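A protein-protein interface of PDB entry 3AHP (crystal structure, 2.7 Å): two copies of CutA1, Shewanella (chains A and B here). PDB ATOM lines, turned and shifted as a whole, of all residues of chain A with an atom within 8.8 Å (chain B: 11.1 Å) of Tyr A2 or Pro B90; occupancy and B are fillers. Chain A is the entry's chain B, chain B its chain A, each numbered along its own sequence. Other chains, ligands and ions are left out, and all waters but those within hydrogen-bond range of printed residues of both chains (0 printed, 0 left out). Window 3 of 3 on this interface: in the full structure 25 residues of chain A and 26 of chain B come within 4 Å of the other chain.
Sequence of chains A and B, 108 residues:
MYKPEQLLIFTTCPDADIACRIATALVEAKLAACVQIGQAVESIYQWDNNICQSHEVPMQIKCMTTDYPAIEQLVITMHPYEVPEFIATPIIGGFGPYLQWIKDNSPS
Phe B10 touches Leu A8.
CD2 of Leu A8 touches CD1 of Ile B87, at 3.8 Å.
Pro A90 touches Ala B88 (O to O, 3.9 Å).
Pro B90 touches Pro A90 (CD to O, 3.4 Å).
CD1 of Ile A91 touches CD1 of Ile B87, at 3.7 Å.
Ile A91 touches Ala B88.
Pro B4 touches Ile A92.
Leu B7 touches Ile A92 (CD2 to CD1, 3.9 Å).
Pro B90 touches Ile A92.
Gly A93 touches Ile B87.
The backbone carbonyl oxygen (O) of Gly A93 lies within hydrogen-bond range of the backbone NH (N) of Ala B88 (2.7 Å).
The backbone NH (N) of Ile A92 sits at hydrogen-bond distance from the backbone carbonyl oxygen (O) of Ala B88, at 3.0 Å.
O of Pro A90 lies within hydrogen-bond range of OG1 of Thr B89 (3.4 Å).
No residue of chain B comes within 4 Å of Lys A3.
No residue of chain B comes within 4 Å of Pro A4.
Of the printed residues of chain B, Ile A91 touches Ile B87 (3.7 Å) and Ala B88 (3.4 Å).
Of the printed residues of chain A, Phe B10 touches Leu A8.
Of the printed residues of chain A, Pro B90 touches Tyr A2, Pro A90 and Ile A92.
Ile B91 touches none of the printed residues of chain A.
The nearest residue of chain B that does not touch Tyr A2 is Pro B4 (4.1 Å).
Thr A89 touches its own counterpart, Thr B89.
Pro A90 touches Thr B89, but with the chains exchanged Thr A89 does not touch Pro B90 (5.9 Å).
Ile A92 touches Leu B7, but with the chains exchanged Leu A7 does not touch Ile B92 (13.6 Å).
Ile A92 touches Pro B90, but with the chains exchanged Pro A90 does not touch Ile B92 (7.4 Å).
The backbone carbonyl oxygen (O) of Pro B4 lies within hydrogen-bond range of the side-chain hydroxyl (OG1) of Thr B65 (2.8 Å).
The backbone carbonyl oxygen of Cys B63 sits at hydrogen-bond distance from the backbone NH of Leu B7.
N of Leu B8 lies within hydrogen-bond range of O of Thr B89 (2.7 Å).
O of Gln A6 sits at hydrogen-bond distance from N of Ile A91, at 3.2 Å.
The backbone carbonyl oxygen of Leu A8 is in hydrogen-bond range of the backbone NH of Thr A89.
The backbone NH of Phe B10 lies within hydrogen-bond range of the backbone carbonyl oxygen of Ile B87, 2.9 Å away.
Of the 13 printed residues of chain A, 7 touch a printed residue of chain B.
Hydrophobic or aromatic side chains of chain B that line the printed part of chain A: Pro B4, Leu B7, Phe B10, Ile B87, Ala B88 and Pro B90.
Among the printed residues, 15 pairs touch across the chains.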
ATOM      1  N   TYR A   2       8.733 -27.357  15.168  1.00  0.00           N
ATOM      2  CA  TYR A   2       8.851 -25.871  15.247  1.00  0.00           C
ATOM      3  C   TYR A   2       8.502 -25.234  13.902  1.00  0.00           C
ATOM      4  O   TYR A   2       8.836 -25.782  12.848  1.00  0.00           O
ATOM      5  CB  TYR A   2      10.274 -25.464  15.662  1.00  0.00           C
ATOM      6  CG  TYR A   2      10.587 -25.686  17.130  1.00  0.00           C
ATOM      7  CD1 TYR A   2      11.576 -26.594  17.527  1.00  0.00           C
ATOM      8  CD2 TYR A   2       9.883 -25.000  18.122  1.00  0.00           C
ATOM      9  CE1 TYR A   2      11.850 -26.819  18.878  1.00  0.00           C
ATOM     10  CE2 TYR A   2      10.146 -25.217  19.478  1.00  0.00           C
ATOM     11  CZ  TYR A   2      11.130 -26.123  19.842  1.00  0.00           C
ATOM     12  OH  TYR A   2      11.389 -26.328  21.169  1.00  0.00           O
ATOM     13  N   LYS A   3       7.834 -24.078  13.942  1.00  0.00           N
ATOM     14  CA  LYS A   3       7.818 -23.154  12.799  1.00  0.00           C
ATOM     15  C   LYS A   3       7.935 -21.677  13.225  1.00  0.00           C
ATOM     16  O   LYS A   3       6.953 -20.938  13.197  1.00  0.00           O
ATOM     17  CB  LYS A   3       6.570 -23.383  11.933  1.00  0.00           C
ATOM     18  CG  LYS A   3       6.610 -22.691  10.565  1.00  0.00           C
ATOM     19  CD  LYS A   3       7.485 -23.439   9.552  1.00  0.00           C
ATOM     20  CE  LYS A   3       6.985 -23.220   8.114  1.00  0.00           C
ATOM     21  NZ  LYS A   3       7.661 -24.115   7.129  1.00  0.00           N
ATOM     22  N   PRO A   4       9.157 -21.238  13.580  1.00  0.00           N
ATOM     23  CA  PRO A   4       9.445 -19.907  14.139  1.00  0.00           C
ATOM     24  C   PRO A   4       9.290 -18.724  13.154  1.00  0.00           C
ATOM     25  O   PRO A   4       9.356 -18.921  11.944  1.00  0.00           O
ATOM     26  CB  PRO A   4      10.903 -20.036  14.586  1.00  0.00           C
ATOM     27  CG  PRO A   4      11.471 -21.135  13.738  1.00  0.00           C
ATOM     28  CD  PRO A   4      10.359 -22.089  13.512  1.00  0.00           C
ATOM     29  N   GLU A   5       9.075 -17.514  13.685  1.00  0.00           N
ATOM     30  CA  GLU A   5       9.063 -16.279  12.879  1.00  0.00           C
ATOM     31  C   GLU A   5      10.450 -16.056  12.323  1.00  0.00           C
ATOM     32  O   GLU A   5      10.622 -15.529  11.220  1.00  0.00           O
ATOM     33  CB  GLU A   5       8.734 -15.041  13.732  1.00  0.00           C
ATOM     34  CG  GLU A   5       7.380 -15.014  14.411  1.00  0.00           C
ATOM     35  CD  GLU A   5       6.250 -15.098  13.418  1.00  0.00           C
ATOM     36  OE1 GLU A   5       6.369 -15.895  12.463  1.00  0.00           O
ATOM     37  OE2 GLU A   5       5.238 -14.392  13.604  1.00  0.00           O
ATOM     38  N   GLN A   6      11.438 -16.336  13.165  1.00  0.00           N
ATOM     39  CA  GLN A   6      12.791 -15.902  12.917  1.00  0.00           C
ATOM     40  C   GLN A   6      13.789 -17.023  13.100  1.00  0.00           C
ATOM     41  O   GLN A   6      13.548 -17.949  13.887  1.00  0.00           O
ATOM     42  CB  GLN A   6      13.132 -14.731  13.818  1.00  0.00           C
ATOM     43  CG  GLN A   6      12.311 -13.501  13.513  1.00  0.00           C
ATOM     44  CD  GLN A   6      11.961 -12.727  14.747  1.00  0.00           C
ATOM     45  OE1 GLN A   6      11.650 -13.304  15.787  1.00  0.00           O
ATOM     46  NE2 GLN A   6      12.050 -11.411  14.657  1.00  0.00           N
ATOM     47  N   LEU A   7      14.886 -16.956  12.339  1.00  0.00           N
ATOM     48  CA  LEU A   7      15.942 -17.952  12.425  1.00  0.00           C
ATOM     49  C   LEU A   7      17.265 -17.376  12.877  1.00  0.00           C
ATOM     50  O   LEU A   7      17.577 -16.227  12.618  1.00  0.00           O
ATOM     51  CB  LEU A   7      16.141 -18.659  11.094  1.00  0.00           C
ATOM     52  CG  LEU A   7      14.921 -19.277  10.421  1.00  0.00           C
ATOM     53  CD1 LEU A   7      15.188 -19.438   8.934  1.00  0.00           C
ATOM     54  CD2 LEU A   7      14.532 -20.600  11.083  1.00  0.00           C
ATOM     55  N   LEU A   8      18.059 -18.224  13.519  1.00  0.00           N
ATOM     56  CA  LEU A   8      19.501 -18.052  13.587  1.00  0.00           C
ATOM     57  C   LEU A   8      20.195 -19.026  12.640  1.00  0.00           C
ATOM     58  O   LEU A   8      20.039 -20.231  12.754  1.00  0.00           O
ATOM     59  CB  LEU A   8      19.967 -18.280  15.023  1.00  0.00           C
ATOM     60  CG  LEU A   8      21.416 -17.981  15.392  1.00  0.00           C
ATOM     61  CD1 LEU A   8      21.746 -16.561  15.054  1.00  0.00           C
ATOM     62  CD2 LEU A   8      21.669 -18.296  16.872  1.00  0.00           C
ATOM     63  N   THR A  65      12.287 -16.008   8.993  1.00  0.00           N
ATOM     64  CA  THR A  65      12.185 -17.282   8.317  1.00  0.00           C
ATOM     65  C   THR A  65      11.691 -17.043   6.909  1.00  0.00           C
ATOM     66  O   THR A  65      11.925 -17.812   5.986  1.00  0.00           O
ATOM     67  CB  THR A  65      11.195 -18.146   9.066  1.00  0.00           C
ATOM     68  OG1 THR A  65      11.723 -18.404  10.368  1.00  0.00           O
ATOM     69  CG2 THR A  65      10.905 -19.446   8.320  1.00  0.00           C
ATOM     70  N   THR A  89      18.951 -22.718  12.963  1.00  0.00           N
ATOM     71  CA  THR A  89      18.284 -23.092  14.205  1.00  0.00           C
ATOM     72  C   THR A  89      17.177 -22.090  14.554  1.00  0.00           C
ATOM     73  O   THR A  89      17.241 -20.932  14.153  1.00  0.00           O
ATOM     74  CB  THR A  89      19.291 -23.172  15.355  1.00  0.00           C
ATOM     75  OG1 THR A  89      19.665 -21.852  15.756  1.00  0.00           O
ATOM     76  CG2 THR A  89      20.548 -23.927  14.906  1.00  0.00           C
ATOM     77  N   PRO A  90      16.143 -22.528  15.293  1.00  0.00           N
ATOM     78  CA  PRO A  90      14.990 -21.659  15.528  1.00  0.00           C
ATOM     79  C   PRO A  90      15.229 -20.676  16.671  1.00  0.00           C
ATOM     80  O   PRO A  90      15.778 -21.053  17.714  1.00  0.00           O
ATOM     81  CB  PRO A  90      13.904 -22.649  15.923  1.00  0.00           C
ATOM     82  CG  PRO A  90      14.664 -23.729  16.637  1.00  0.00           C
ATOM     83  CD  PRO A  90      15.972 -23.853  15.913  1.00  0.00           C
ATOM     84  N   ILE A  91      14.877 -19.412  16.452  1.00  0.00           N
ATOM     85  CA  ILE A  91      14.773 -18.460  17.544  1.00  0.00           C
ATOM     86  C   ILE A  91      13.376 -18.562  18.137  1.00  0.00           C
ATOM     87  O   ILE A  91      12.400 -18.334  17.438  1.00  0.00           O
ATOM     88  CB  ILE A  91      14.985 -17.024  17.061  1.00  0.00           C
ATOM     89  CG1 ILE A  91      16.459 -16.775  16.740  1.00  0.00           C
ATOM     90  CG2 ILE A  91      14.504 -16.048  18.121  1.00  0.00           C
ATOM     91  CD1 ILE A  91      16.721 -15.464  16.016  1.00  0.00           C
ATOM     92  N   ILE A  92      13.271 -18.927  19.411  1.00  0.00           N
ATOM     93  CA  ILE A  92      11.958 -19.007  20.046  1.00  0.00           C
ATOM     94  C   ILE A  92      11.699 -17.887  21.050  1.00  0.00           C
ATOM     95  O   ILE A  92      10.686 -17.893  21.740  1.00  0.00           O
ATOM     96  CB  ILE A  92      11.694 -20.381  20.701  1.00  0.00           C
ATOM     97  CG1 ILE A  92      12.568 -20.559  21.944  1.00  0.00           C
ATOM     98  CG2 ILE A  92      11.907 -21.509  19.701  1.00  0.00           C
ATOM     99  CD1 ILE A  92      12.810 -22.005  22.337  1.00  0.00           C
ATOM    100  N   GLY A  93      12.601 -16.916  21.131  1.00  0.00           N
ATOM    101  CA  GLY A  93      12.463 -15.872  22.129  1.00  0.00           C
ATOM    102  C   GLY A  93      13.510 -14.803  21.966  1.00  0.00           C
ATOM    103  O   GLY A  93      14.504 -14.995  21.266  1.00  0.00           O
ATOM    104  N   LYS B   3       7.702 -26.860  24.392  1.00  0.00           N
ATOM    105  CA  LYS B   3       8.461 -25.682  24.899  1.00  0.00           C
ATOM    106  C   LYS B   3       9.515 -26.083  25.938  1.00  0.00           C
ATOM    107  O   LYS B   3       9.192 -26.696  26.939  1.00  0.00           O
ATOM    108  CB  LYS B   3       7.497 -24.620  25.455  1.00  0.00           C
ATOM    109  CG  LYS B   3       6.587 -23.990  24.378  1.00  0.00           C
ATOM    110  CD  LYS B   3       7.214 -24.079  22.962  1.00  0.00           C
ATOM    111  CE  LYS B   3       7.511 -22.700  22.355  1.00  0.00           C
ATOM    112  NZ  LYS B   3       8.535 -21.933  23.124  1.00  0.00           N
ATOM    113  N   PRO B   4      10.785 -25.744  25.687  1.00  0.00           N
ATOM    114  CA  PRO B   4      11.929 -26.378  26.351  1.00  0.00           C
ATOM    115  C   PRO B   4      12.052 -26.058  27.843  1.00  0.00           C
ATOM    116  O   PRO B   4      11.661 -24.974  28.283  1.00  0.00           O
ATOM    117  CB  PRO B   4      13.121 -25.796  25.605  1.00  0.00           C
ATOM    118  CG  PRO B   4      12.660 -24.481  25.134  1.00  0.00           C
ATOM    119  CD  PRO B   4      11.186 -24.563  24.905  1.00  0.00           C
ATOM    120  N   GLU B   5      12.624 -26.983  28.607  1.00  0.00           N
ATOM    121  CA  GLU B   5      13.039 -26.665  29.965  1.00  0.00           C
ATOM    122  C   GLU B   5      14.189 -25.656  29.968  1.00  0.00           C
ATOM    123  O   GLU B   5      14.236 -24.771  30.808  1.00  0.00           O
ATOM    124  CB  GLU B   5      13.418 -27.924  30.740  1.00  0.00           C
ATOM    125  CG  GLU B   5      12.409 -28.298  31.817  1.00  0.00           C
ATOM    126  CD  GLU B   5      13.077 -28.789  33.103  1.00  0.00           C
ATOM    127  OE1 GLU B   5      13.703 -29.877  33.073  1.00  0.00           O
ATOM    128  OE2 GLU B   5      12.969 -28.099  34.149  1.00  0.00           O
ATOM    129  N   GLN B   6      15.074 -25.737  28.982  1.00  0.00           N
ATOM    130  CA  GLN B   6      16.275 -24.907  28.999  1.00  0.00           C
ATOM    131  C   GLN B   6      16.584 -24.150  27.715  1.00  0.00           C
ATOM    132  O   GLN B   6      16.134 -24.523  26.653  1.00  0.00           O
ATOM    133  CB  GLN B   6      17.467 -25.716  29.477  1.00  0.00           C
ATOM    134  CG  GLN B   6      17.191 -26.359  30.801  1.00  0.00           C
ATOM    135  CD  GLN B   6      18.022 -27.570  31.021  1.00  0.00           C
ATOM    136  OE1 GLN B   6      18.767 -27.651  31.998  1.00  0.00           O
ATOM    137  NE2 GLN B   6      17.911 -28.534  30.115  1.00  0.00           N
ATOM    138  N   LEU B   7      17.299 -23.037  27.849  1.00  0.00           N
ATOM    139  CA  LEU B   7      17.611 -22.172  26.717  1.00  0.00           C
ATOM    140  C   LEU B   7      19.097 -21.895  26.545  1.00  0.00           C
ATOM    141  O   LEU B   7      19.865 -21.848  27.519  1.00  0.00           O
ATOM    142  CB  LEU B   7      16.859 -20.844  26.803  1.00  0.00           C
ATOM    143  CG  LEU B   7      15.340 -20.894  26.848  1.00  0.00           C
ATOM    144  CD1 LEU B   7      14.771 -19.488  26.946  1.00  0.00           C
ATOM    145  CD2 LEU B   7      14.752 -21.674  25.671  1.00  0.00           C
ATOM    146  N   LEU B   8      19.476 -21.667  25.290  1.00  0.00           N
ATOM    147  CA  LEU B   8      20.777 -21.095  24.948  1.00  0.00           C
ATOM    148  C   LEU B   8      20.541 -19.690  24.414  1.00  0.00           C
ATOM    149  O   LEU B   8      19.783 -19.510  23.473  1.00  0.00           O
ATOM    150  CB  LEU B   8      21.452 -21.968  23.886  1.00  0.00           C
ATOM    151  CG  LEU B   8      22.901 -21.653  23.515  1.00  0.00           C
ATOM    152  CD1 LEU B   8      23.812 -21.686  24.750  1.00  0.00           C
ATOM    153  CD2 LEU B   8      23.392 -22.595  22.422  1.00  0.00           C
ATOM    154  N   ILE B   9      21.059 -18.685  25.106  1.00  0.00           N
ATOM    155  CA  ILE B   9      20.790 -17.297  24.748  1.00  0.00           C
ATOM    156  C   ILE B   9      22.033 -16.664  24.139  1.00  0.00           C
ATOM    157  O   ILE B   9      23.118 -16.737  24.723  1.00  0.00           O
ATOM    158  CB  ILE B   9      20.399 -16.465  25.988  1.00  0.00           C
ATOM    159  CG1 ILE B   9      19.131 -17.013  26.643  1.00  0.00           C
ATOM    160  CG2 ILE B   9      20.216 -14.993  25.629  1.00  0.00           C
ATOM    161  CD1 ILE B   9      18.692 -16.182  27.820  1.00  0.00           C
ATOM    162  N   PHE B  10      21.874 -16.041  22.976  1.00  0.00           N
ATOM    163  CA  PHE B  10      22.970 -15.327  22.337  1.00  0.00           C
ATOM    164  C   PHE B  10      22.830 -13.817  22.532  1.00  0.00           C
ATOM    165  O   PHE B  10      21.746 -13.238  22.410  1.00  0.00           O
ATOM    166  CB  PHE B  10      23.072 -15.669  20.832  1.00  0.00           C
ATOM    167  CG  PHE B  10      23.385 -17.119  20.551  1.00  0.00           C
ATOM    168  CD1 PHE B  10      22.367 -18.072  20.500  1.00  0.00           C
ATOM    169  CD2 PHE B  10      24.699 -17.540  20.388  1.00  0.00           C
ATOM    170  CE1 PHE B  10      22.653 -19.405  20.271  1.00  0.00           C
ATOM    171  CE2 PHE B  10      24.994 -18.869  20.125  1.00  0.00           C
ATOM    172  CZ  PHE B  10      23.969 -19.798  20.057  1.00  0.00           C
ATOM    173  N   GLN B  60      27.267 -16.220  25.300  1.00  0.00           N
ATOM    174  CA  GLN B  60      26.303 -17.308  25.387  1.00  0.00           C
ATOM    175  C   GLN B  60      25.910 -17.603  26.833  1.00  0.00           C
ATOM    176  O   GLN B  60      26.765 -17.885  27.674  1.00  0.00           O
ATOM    177  CB  GLN B  60      26.892 -18.576  24.796  1.00  0.00           C
ATOM    178  CG  GLN B  60      26.912 -18.639  23.306  1.00  0.00           C
ATOM    179  CD  GLN B  60      27.511 -19.945  22.841  1.00  0.00           C
ATOM    180  OE1 GLN B  60      27.534 -20.933  23.607  1.00  0.00           O
ATOM    181  NE2 GLN B  60      28.087 -19.942  21.632  1.00  0.00           N
ATOM    182  N   ILE B  61      24.608 -17.670  27.072  1.00  0.00           N
ATOM    183  CA  ILE B  61      24.085 -17.861  28.403  1.00  0.00           C
ATOM    184  C   ILE B  61      23.295 -19.154  28.433  1.00  0.00           C
ATOM    185  O   ILE B  61      22.412 -19.375  27.601  1.00  0.00           O
ATOM    186  CB  ILE B  61      23.144 -16.708  28.769  1.00  0.00           C
ATOM    187  CG1 ILE B  61      23.936 -15.408  28.931  1.00  0.00           C
ATOM    188  CG2 ILE B  61      22.283 -17.058  29.976  1.00  0.00           C
ATOM    189  CD1 ILE B  61      23.164 -14.185  28.496  1.00  0.00           C
ATOM    190  N   LYS B  62      23.656 -20.035  29.361  1.00  0.00           N
ATOM    191  CA  LYS B  62      22.915 -21.272  29.561  1.00  0.00           C
ATOM    192  C   LYS B  62      22.096 -21.157  30.829  1.00  0.00           C
ATOM    193  O   LYS B  62      22.597 -20.756  31.871  1.00  0.00           O
ATOM    194  CB  LYS B  62      23.854 -22.478  29.626  1.00  0.00           C
ATOM    195  CG  LYS B  62      24.458 -22.864  28.293  1.00  0.00           C
ATOM    196  CD  LYS B  62      25.965 -23.040  28.393  1.00  0.00           C
ATOM    197  CE  LYS B  62      26.708 -21.722  28.231  1.00  0.00           C
ATOM    198  NZ  LYS B  62      28.123 -21.955  27.828  1.00  0.00           N
ATOM    199  N   CYS B  63      20.816 -21.465  30.719  1.00  0.00           N
ATOM    200  CA  CYS B  63      19.875 -21.061  31.722  1.00  0.00           C
ATOM    201  C   CYS B  63      18.586 -21.860  31.607  1.00  0.00           C
ATOM    202  O   CYS B  63      18.326 -22.507  30.589  1.00  0.00           O
ATOM    203  CB  CYS B  63      19.581 -19.579  31.556  1.00  0.00           C
ATOM    204  SG  CYS B  63      18.404 -19.223  30.250  1.00  0.00           S
ATOM    205  N   MET B  64      17.767 -21.779  32.652  1.00  0.00           N
ATOM    206  CA  MET B  64      16.428 -22.352  32.627  1.00  0.00           C
ATOM    207  C   MET B  64      15.458 -21.362  31.996  1.00  0.00           C
ATOM    208  O   MET B  64      15.571 -20.161  32.213  1.00  0.00           O
ATOM    209  CB  MET B  64      15.983 -22.706  34.049  1.00  0.00           C
ATOM    210  CG  MET B  64      16.977 -23.577  34.823  1.00  0.00           C
ATOM    211  SD  MET B  64      16.886 -25.298  34.304  1.00  0.00           S
ATOM    212  CE  MET B  64      15.111 -25.574  34.324  1.00  0.00           C
ATOM    213  N   THR B  65      14.599 -21.862  31.110  1.00  0.00           N
ATOM    214  CA  THR B  65      13.575 -21.050  30.451  1.00  0.00           C
ATOM    215  C   THR B  65      12.804 -20.228  31.474  1.00  0.00           C
ATOM    216  O   THR B  65      12.491 -19.054  31.277  1.00  0.00           O
ATOM    217  CB  THR B  65      12.591 -21.958  29.732  1.00  0.00           C
ATOM    218  OG1 THR B  65      13.305 -22.748  28.787  1.00  0.00           O
ATOM    219  CG2 THR B  65      11.497 -21.159  29.048  1.00  0.00           C
ATOM    220  N   TYR B  68      14.023 -16.853  32.295  1.00  0.00           N
ATOM    221  CA  TYR B  68      14.294 -15.994  31.135  1.00  0.00           C
ATOM    222  C   TYR B  68      13.934 -14.506  31.328  1.00  0.00           C
ATOM    223  O   TYR B  68      14.710 -13.617  30.946  1.00  0.00           O
ATOM    224  CB  TYR B  68      13.637 -16.534  29.854  1.00  0.00           C
ATOM    225  CG  TYR B  68      13.689 -15.539  28.703  1.00  0.00           C
ATOM    226  CD1 TYR B  68      14.746 -15.554  27.796  1.00  0.00           C
ATOM    227  CD2 TYR B  68      12.740 -14.520  28.589  1.00  0.00           C
ATOM    228  CE1 TYR B  68      14.840 -14.605  26.801  1.00  0.00           C
ATOM    229  CE2 TYR B  68      12.816 -13.589  27.570  1.00  0.00           C
ATOM    230  CZ  TYR B  68      13.872 -13.641  26.687  1.00  0.00           C
ATOM    231  OH  TYR B  68      13.989 -12.699  25.711  1.00  0.00           O
ATOM    232  N   ILE B  87      18.780 -13.061  21.869  1.00  0.00           N
ATOM    233  CA  ILE B  87      17.907 -14.047  21.248  1.00  0.00           C
ATOM    234  C   ILE B  87      17.957 -15.399  21.952  1.00  0.00           C
ATOM    235  O   ILE B  87      18.989 -15.806  22.475  1.00  0.00           O
ATOM    236  CB  ILE B  87      18.168 -14.201  19.732  1.00  0.00           C
ATOM    237  CG1 ILE B  87      19.600 -14.647  19.481  1.00  0.00           C
ATOM    238  CG2 ILE B  87      17.897 -12.893  19.001  1.00  0.00           C
ATOM    239  CD1 ILE B  87      19.814 -15.222  18.105  1.00  0.00           C
ATOM    240  N   ALA B  88      16.811 -16.057  22.023  1.00  0.00           N
ATOM    241  CA  ALA B  88      16.732 -17.350  22.669  1.00  0.00           C
ATOM    242  C   ALA B  88      16.678 -18.510  21.677  1.00  0.00           C
ATOM    243  O   ALA B  88      15.909 -18.504  20.726  1.00  0.00           O
ATOM    244  CB  ALA B  88      15.532 -17.393  23.608  1.00  0.00           C
ATOM    245  N   THR B  89      17.414 -19.554  22.014  1.00  0.00           N
ATOM    246  CA  THR B  89      17.451 -20.795  21.266  1.00  0.00           C
ATOM    247  C   THR B  89      17.158 -22.001  22.197  1.00  0.00           C
ATOM    248  O   THR B  89      17.576 -22.021  23.369  1.00  0.00           O
ATOM    249  CB  THR B  89      18.823 -20.922  20.601  1.00  0.00           C
ATOM    250  OG1 THR B  89      18.723 -20.488  19.242  1.00  0.00           O
ATOM    251  CG2 THR B  89      19.348 -22.329  20.655  1.00  0.00           C
ATOM    252  N   PRO B  90      16.413 -22.998  21.694  1.00  0.00           N
ATOM    253  CA  PRO B  90      16.061 -24.130  22.542  1.00  0.00           C
ATOM    254  C   PRO B  90      17.253 -25.055  22.804  1.00  0.00           C
ATOM    255  O   PRO B  90      18.010 -25.385  21.884  1.00  0.00           O
ATOM    256  CB  PRO B  90      14.992 -24.870  21.721  1.00  0.00           C
ATOM    257  CG  PRO B  90      14.986 -24.253  20.350  1.00  0.00           C
ATOM    258  CD  PRO B  90      16.111 -23.263  20.280  1.00  0.00           C
ATOM    259  N   ILE B  91      17.414 -25.477  24.047  1.00  0.00           N
ATOM    260  CA  ILE B  91      18.176 -26.675  24.312  1.00  0.00           C
ATOM    261  C   ILE B  91      17.220 -27.849  24.348  1.00  0.00           C
ATOM    262  O   ILE B  91      16.179 -27.770  24.982  1.00  0.00           O
ATOM    263  CB  ILE B  91      18.942 -26.575  25.625  1.00  0.00           C
ATOM    264  CG1 ILE B  91      20.155 -25.672  25.423  1.00  0.00           C
ATOM    265  CG2 ILE B  91      19.371 -27.955  26.107  1.00  0.00           C
ATOM    266  CD1 ILE B  91      20.602 -24.959  26.665  1.00  0.00           C
ATOM    267  N   ILE B  92      17.540 -28.905  23.601  1.00  0.00           N
ATOM    268  CA  ILE B  92      16.684 -30.073  23.548  1.00  0.00           C
ATOM    269  C   ILE B  92      17.440 -31.353  23.863  1.00  0.00           C
ATOM    270  O   ILE B  92      16.943 -32.440  23.642  1.00  0.00           O
ATOM    271  CB  ILE B  92      16.034 -30.221  22.170  1.00  0.00           C
ATOM    272  CG1 ILE B  92      17.096 -30.528  21.121  1.00  0.00           C
ATOM    273  CG2 ILE B  92      15.220 -28.972  21.804  1.00  0.00           C
ATOM    274  CD1 ILE B  92      16.559 -31.322  20.013  1.00  0.00           C
ATOM    275  N   GLY B  93      18.683 -31.233  24.292  1.00  0.00           N
ATOM    276  CA  GLY B  93      19.381 -32.394  24.774  1.00  0.00           C
ATOM    277  C   GLY B  93      20.697 -31.964  25.343  1.00  0.00           C
ATOM    278  O   GLY B  93      21.092 -30.810  25.211  1.00  0.00           O
ATOM    279  N   GLY B  94      21.374 -32.900  25.984  1.00  0.00           N
ATOM    280  CA  GLY B  94      22.730 -32.692  26.449  1.00  0.00           C
ATOM    281  C   GLY B  94      23.070 -33.839  27.362  1.00  0.00           C
ATOM    282  O   GLY B  94      22.235 -34.686  27.600  1.00  0.00           O
ATOM    283  N   LEU B  99      22.841 -30.882  32.227  1.00  0.00           N
ATOM    284  CA  LEU B  99      21.498 -30.302  32.233  1.00  0.00           C
ATOM    285  C   LEU B  99      21.002 -30.197  33.661  1.00  0.00           C
ATOM    286  O   LEU B  99      20.438 -29.163  34.042  1.00  0.00           O
ATOM    287  CB  LEU B  99      20.500 -31.118  31.386  1.00  0.00           C
ATOM    288  CG  LEU B  99      20.834 -31.371  29.900  1.00  0.00           C
ATOM    289  CD1 LEU B  99      19.661 -31.953  29.133  1.00  0.00           C
ATOM    290  CD2 LEU B  99      21.408 -30.151  29.181  1.00  0.00           C
ATOM    291  N   ILE B 102      22.579 -27.255  35.547  1.00  0.00           N
ATOM    292  CA  ILE B 102      21.843 -26.042  35.172  1.00  0.00           C
ATOM    293  C   ILE B 102      20.555 -25.889  35.963  1.00  0.00           C
ATOM    294  O   ILE B 102      20.251 -24.806  36.433  1.00  0.00           O
ATOM    295  CB  ILE B 102      21.512 -26.004  33.662  1.00  0.00           C
ATOM    296  CG1 ILE B 102      22.792 -25.954  32.831  1.00  0.00           C
ATOM    297  CG2 ILE B 102      20.647 -24.795  33.313  1.00  0.00           C
ATOM    298  CD1 ILE B 102      22.550 -25.961  31.353  1.00  0.00           C
